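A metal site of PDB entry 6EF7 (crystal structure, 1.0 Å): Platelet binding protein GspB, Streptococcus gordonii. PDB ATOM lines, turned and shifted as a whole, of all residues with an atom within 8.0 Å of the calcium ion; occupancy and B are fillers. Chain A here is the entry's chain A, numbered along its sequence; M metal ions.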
ATOM      1  N   SER A   4     -14.608 -20.238  16.390  1.00  0.00           N
ATOM      2  CA  SER A   4     -13.486 -19.330  16.214  1.00  0.00           C
ATOM      3  C   SER A   4     -13.029 -19.334  14.760  1.00  0.00           C
ATOM      4  O   SER A   4     -13.172 -20.312  14.034  1.00  0.00           O
ATOM      5  CB  SER A   4     -12.314 -19.727  17.109  1.00  0.00           C
ATOM      6  OG  SER A   4     -11.688 -20.892  16.623  1.00  0.00           O
ATOM      7  N   ASP A   5     -12.479 -18.203  14.326  1.00  0.00           N
ATOM      8  CA  ASP A   5     -12.077 -18.034  12.932  1.00  0.00           C
ATOM      9  C   ASP A   5     -10.866 -17.110  12.895  1.00  0.00           C
ATOM     10  O   ASP A   5     -11.011 -15.888  13.057  1.00  0.00           O
ATOM     11  CB  ASP A   5     -13.220 -17.464  12.120  1.00  0.00           C
ATOM     12  CG  ASP A   5     -12.854 -17.270  10.653  1.00  0.00           C
ATOM     13  OD1 ASP A   5     -11.716 -17.609  10.251  1.00  0.00           O
ATOM     14  OD2 ASP A   5     -13.712 -16.773   9.910  1.00  0.00           O
ATOM     15  N   THR A   6      -9.700 -17.680  12.641  1.00  0.00           N
ATOM     16  CA  THR A   6      -8.461 -16.913  12.566  1.00  0.00           C
ATOM     17  C   THR A   6      -7.867 -16.927  11.159  1.00  0.00           C
ATOM     18  O   THR A   6      -6.717 -16.496  10.981  1.00  0.00           O
ATOM     19  CB  THR A   6      -7.449 -17.452  13.581  1.00  0.00           C
ATOM     20  OG1 THR A   6      -7.212 -18.834  13.328  1.00  0.00           O
ATOM     21  CG2 THR A   6      -7.964 -17.260  15.013  1.00  0.00           C
ATOM     22  N   GLU A   7      -8.614 -17.391  10.163  1.00  0.00           N
ATOM     23  CA  GLU A   7      -8.144 -17.528   8.782  1.00  0.00           C
ATOM     24  C   GLU A   7      -8.725 -16.411   7.927  1.00  0.00           C
ATOM     25  O   GLU A   7      -9.930 -16.136   7.991  1.00  0.00           O
ATOM     26  CB  GLU A   7      -8.549 -18.897   8.221  1.00  0.00           C
ATOM     27  CG  GLU A   7      -8.175 -19.103   6.765  1.00  0.00           C
ATOM     28  CD  GLU A   7      -8.642 -20.433   6.206  1.00  0.00           C
ATOM     29  OE1 GLU A   7      -8.705 -21.411   6.994  1.00  0.00           O
ATOM     30  OE2 GLU A   7      -8.985 -20.499   5.010  1.00  0.00           O
ATOM     31  N   ARG A   8      -7.887 -15.806   7.102  1.00  0.00           N
ATOM     32  CA  ARG A   8      -8.327 -14.674   6.293  1.00  0.00           C
ATOM     33  C   ARG A   8      -9.159 -15.128   5.080  1.00  0.00           C
ATOM     34  O   ARG A   8      -8.875 -16.164   4.468  1.00  0.00           O
ATOM     35  CB  ARG A   8      -7.109 -13.941   5.767  1.00  0.00           C
ATOM     36  CG  ARG A   8      -6.238 -13.273   6.806  1.00  0.00           C
ATOM     37  CD  ARG A   8      -5.032 -12.693   6.116  1.00  0.00           C
ATOM     38  NE  ARG A   8      -4.158 -11.956   7.009  1.00  0.00           N
ATOM     39  CZ  ARG A   8      -3.301 -11.019   6.600  1.00  0.00           C
ATOM     40  NH1 ARG A   8      -3.266 -10.619   5.335  1.00  0.00           N
ATOM     41  NH2 ARG A   8      -2.440 -10.472   7.456  1.00  0.00           N
ATOM     42  N   PRO A   9     -10.119 -14.309   4.663  1.00  0.00           N
ATOM     43  CA  PRO A   9     -10.817 -14.561   3.403  1.00  0.00           C
ATOM     44  C   PRO A   9      -9.843 -14.408   2.235  1.00  0.00           C
ATOM     45  O   PRO A   9      -8.806 -13.738   2.359  1.00  0.00           O
ATOM     46  CB  PRO A   9     -11.914 -13.487   3.385  1.00  0.00           C
ATOM     47  CG  PRO A   9     -11.308 -12.342   4.177  1.00  0.00           C
ATOM     48  CD  PRO A   9     -10.529 -13.020   5.267  1.00  0.00           C
ATOM     49  N   VAL A  10     -10.204 -15.012   1.092  1.00  0.00           N
ATOM     50  CA  VAL A  10      -9.344 -15.018  -0.088  1.00  0.00           C
ATOM     51  C   VAL A  10     -10.101 -14.426  -1.272  1.00  0.00           C
ATOM     52  O   VAL A  10     -11.159 -14.928  -1.649  1.00  0.00           O
ATOM     53  CB  VAL A  10      -8.859 -16.443  -0.430  1.00  0.00           C
ATOM     54  CG1 VAL A  10      -7.990 -16.403  -1.679  1.00  0.00           C
ATOM     55  CG2 VAL A  10      -8.110 -17.084   0.733  1.00  0.00           C
ATOM     56  N   THR A  32     -13.943 -16.037  -1.073  1.00  0.00           N
ATOM     57  CA  THR A  32     -14.291 -17.192  -0.254  1.00  0.00           C
ATOM     58  C   THR A  32     -13.758 -16.985   1.158  1.00  0.00           C
ATOM     59  O   THR A  32     -12.863 -16.162   1.385  1.00  0.00           O
ATOM     60  CB  THR A  32     -13.720 -18.509  -0.833  1.00  0.00           C
ATOM     61  OG1 THR A  32     -12.300 -18.369  -0.992  1.00  0.00           O
ATOM     62  CG2 THR A  32     -14.367 -18.877  -2.182  1.00  0.00           C
ATOM     63  N   ASP A  33     -14.311 -17.739   2.096  1.00  0.00           N
ATOM     64  CA  ASP A  33     -13.783 -17.757   3.455  1.00  0.00           C
ATOM     65  C   ASP A  33     -14.093 -19.100   4.089  1.00  0.00           C
ATOM     66  O   ASP A  33     -15.164 -19.677   3.867  1.00  0.00           O
ATOM     67  CB  ASP A  33     -14.393 -16.658   4.337  1.00  0.00           C
ATOM     68  CG  ASP A  33     -13.664 -16.530   5.661  1.00  0.00           C
ATOM     69  OD1 ASP A  33     -12.471 -16.146   5.633  1.00  0.00           O
ATOM     70  OD2 ASP A  33     -14.233 -16.894   6.726  1.00  0.00           O
ATOM     71  N   ASN A  34     -13.193 -19.564   4.951  1.00  0.00           N
ATOM     72  CA  ASN A  34     -13.412 -20.820   5.668  1.00  0.00           C
ATOM     73  C   ASN A  34     -14.729 -20.838   6.427  1.00  0.00           C
ATOM     74  O   ASN A  34     -15.324 -21.914   6.594  1.00  0.00           O
ATOM     75  CB  ASN A  34     -12.247 -21.110   6.621  1.00  0.00           C
ATOM     76  CG  ASN A  34     -12.043 -20.047   7.662  1.00  0.00           C
ATOM     77  OD1 ASN A  34     -11.919 -18.867   7.328  1.00  0.00           O
ATOM     78  ND2 ASN A  34     -11.989 -20.430   8.914  1.00  0.00           N
ATOM     79  N   SER A  35     -15.165 -19.692   6.961  1.00  0.00           N
ATOM     80  CA  SER A  35     -16.396 -19.641   7.741  1.00  0.00           C
ATOM     81  C   SER A  35     -17.647 -19.506   6.883  1.00  0.00           C
ATOM     82  O   SER A  35     -18.760 -19.635   7.407  1.00  0.00           O
ATOM     83  CB  SER A  35     -16.376 -18.426   8.671  1.00  0.00           C
ATOM     84  OG  SER A  35     -16.610 -17.211   7.941  1.00  0.00           O
ATOM     85  N   ASN A  36     -17.487 -19.191   5.600  1.00  0.00           N
ATOM     86  CA  ASN A  36     -18.605 -18.928   4.685  1.00  0.00           C
ATOM     87  C   ASN A  36     -19.440 -17.708   5.108  1.00  0.00           C
ATOM     88  O   ASN A  36     -20.549 -17.521   4.608  1.00  0.00           O
ATOM     89  CB  ASN A  36     -19.464 -20.176   4.467  1.00  0.00           C
ATOM     90  CG  ASN A  36     -18.666 -21.329   3.902  1.00  0.00           C
ATOM     91  OD1 ASN A  36     -17.814 -21.142   3.036  1.00  0.00           O
ATOM     92  ND2 ASN A  36     -18.917 -22.538   4.402  1.00  0.00           N
ATOM     93  N   ALA A  37     -18.894 -16.856   5.988  1.00  0.00           N
ATOM     94  CA  ALA A  37     -19.608 -15.711   6.518  1.00  0.00           C
ATOM     95  C   ALA A  37     -18.724 -14.475   6.433  1.00  0.00           C
ATOM     96  O   ALA A  37     -17.524 -14.532   6.727  1.00  0.00           O
ATOM     97  CB  ALA A  37     -20.012 -15.956   7.978  1.00  0.00           C
ATOM     98  N   PHE A  38     -19.325 -13.362   6.017  1.00  0.00           N
ATOM     99  CA  PHE A  38     -18.573 -12.178   5.627  1.00  0.00           C
ATOM    100  C   PHE A  38     -19.095 -10.935   6.322  1.00  0.00           C
ATOM    101  O   PHE A  38     -20.160 -10.929   6.922  1.00  0.00           O
ATOM    102  CB  PHE A  38     -18.685 -11.969   4.109  1.00  0.00           C
ATOM    103  CG  PHE A  38     -18.162 -13.133   3.317  1.00  0.00           C
ATOM    104  CD1 PHE A  38     -16.816 -13.231   2.998  1.00  0.00           C
ATOM    105  CD2 PHE A  38     -19.006 -14.158   2.920  1.00  0.00           C
ATOM    106  CE1 PHE A  38     -16.355 -14.315   2.269  1.00  0.00           C
ATOM    107  CE2 PHE A  38     -18.547 -15.232   2.218  1.00  0.00           C
ATOM    108  CZ  PHE A  38     -17.235 -15.317   1.875  1.00  0.00           C
ATOM    109  N   THR A  95     -13.488  -8.500   4.130  1.00  0.00           N
ATOM    110  CA  THR A  95     -13.514  -8.771   5.560  1.00  0.00           C
ATOM    111  C   THR A  95     -14.481  -9.923   5.811  1.00  0.00           C
ATOM    112  O   THR A  95     -15.607  -9.913   5.292  1.00  0.00           O
ATOM    113  CB  THR A  95     -13.989  -7.513   6.322  1.00  0.00           C
ATOM    114  OG1 THR A  95     -13.169  -6.389   5.976  1.00  0.00           O
ATOM    115  CG2 THR A  95     -13.901  -7.706   7.817  1.00  0.00           C
ATOM    116  N   ASP A  96     -14.054 -10.921   6.592  1.00  0.00           N
ATOM    117  CA  ASP A  96     -14.975 -11.971   7.014  1.00  0.00           C
ATOM    118  C   ASP A  96     -15.797 -11.503   8.216  1.00  0.00           C
ATOM    119  O   ASP A  96     -15.608 -10.419   8.764  1.00  0.00           O
ATOM    120  CB  ASP A  96     -14.259 -13.333   7.200  1.00  0.00           C
ATOM    121  CG  ASP A  96     -13.339 -13.389   8.391  1.00  0.00           C
ATOM    122  OD1 ASP A  96     -13.414 -12.528   9.276  1.00  0.00           O
ATOM    123  OD2 ASP A  96     -12.508 -14.349   8.432  1.00  0.00           O
ATOM    124  N   ALA A  97     -16.777 -12.319   8.614  1.00  0.00           N
ATOM    125  CA  ALA A  97     -17.666 -11.914   9.696  1.00  0.00           C
ATOM    126  C   ALA A  97     -16.915 -11.707  11.008  1.00  0.00           C
ATOM    127  O   ALA A  97     -17.338 -10.900  11.843  1.00  0.00           O
ATOM    128  CB  ALA A  97     -18.801 -12.929   9.850  1.00  0.00           C
ATOM    129  N   ALA A  98     -15.823 -12.438  11.208  1.00  0.00           N
ATOM    130  CA  ALA A  98     -14.993 -12.340  12.410  1.00  0.00           C
ATOM    131  C   ALA A  98     -14.034 -11.157  12.381  1.00  0.00           C
ATOM    132  O   ALA A  98     -13.342 -10.923  13.382  1.00  0.00           O
ATOM    133  CB  ALA A  98     -14.195 -13.618  12.580  1.00  0.00           C
ATOM    134  N   GLY A  99     -13.948 -10.432  11.273  1.00  0.00           N
ATOM    135  CA  GLY A  99     -13.090  -9.258  11.185  1.00  0.00           C
ATOM    136  C   GLY A  99     -11.733  -9.478  10.548  1.00  0.00           C
ATOM    137  O   GLY A  99     -10.941  -8.533  10.478  1.00  0.00           O
ATOM    138  N   ASN A 100     -11.413 -10.700  10.115  1.00  0.00           N
ATOM    139  CA  ASN A 100     -10.163 -10.905   9.387  1.00  0.00           C
ATOM    140  C   ASN A 100     -10.273 -10.299   7.986  1.00  0.00           C
ATOM    141  O   ASN A 100     -11.338 -10.370   7.358  1.00  0.00           O
ATOM    142  CB  ASN A 100      -9.866 -12.402   9.242  1.00  0.00           C
ATOM    143  CG  ASN A 100      -9.819 -13.125  10.566  1.00  0.00           C
ATOM    144  OD1 ASN A 100      -8.886 -12.905  11.361  1.00  0.00           O
ATOM    145  ND2 ASN A 100     -10.785 -13.997  10.797  1.00  0.00           N
ATOM    146  N   VAL A 101      -9.164  -9.748   7.502  1.00  0.00           N
ATOM    147  CA  VAL A 101      -9.084  -9.159   6.171  1.00  0.00           C
ATOM    148  C   VAL A 101      -8.032  -9.886   5.337  1.00  0.00           C
ATOM    149  O   VAL A 101      -7.037 -10.396   5.862  1.00  0.00           O
ATOM    150  CB  VAL A 101      -8.778  -7.640   6.206  1.00  0.00           C
ATOM    151  CG1 VAL A 101      -9.875  -6.897   6.932  1.00  0.00           C
ATOM    152  CG2 VAL A 101      -7.410  -7.344   6.832  1.00  0.00           C
HETATM  153 CA    CA M   1     -12.183 -16.608   8.019  1.00  0.00          CA
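The side-chain carboxylate of Asp 33 lies close to the side-chain hydroxyl of Ser 35. N of Gly 99 is in hydrogen-bond range of OD1 of Asp 96. The backbone carbonyl oxygen of Asp 5 is in hydrogen-bond range of the side-chain amide nitrogen of Asn 100 (3.0 Å). The side-chain amide oxygen of Asn 36 lies close to the backbone carbonyl oxygen of Asp 33 (3.1 Å). The side-chain carboxylate (OD1) of Asp 96 sits at hydrogen-bond distance from the backbone NH (N) of Ala 98. The side-chain carboxylate (OD1) of Asp 96 lies within hydrogen-bond range of the backbone NH (N) of Asn 100 (2.8 Å).
The calcium ion is bound by O of Glu 7 (2.3 Å), OD2 of Asp 96 (2.3 Å), OD1 of Asn 34 (2.4 Å), OD2 of Asp 5 (2.4 Å), OD2 of Asp 33 (2.4 Å), OD1 of Asp 33 (2.4 Å) and OD1 of Asp 5 (2.5 Å). The calcium ion has seven donor atoms within binding distance.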
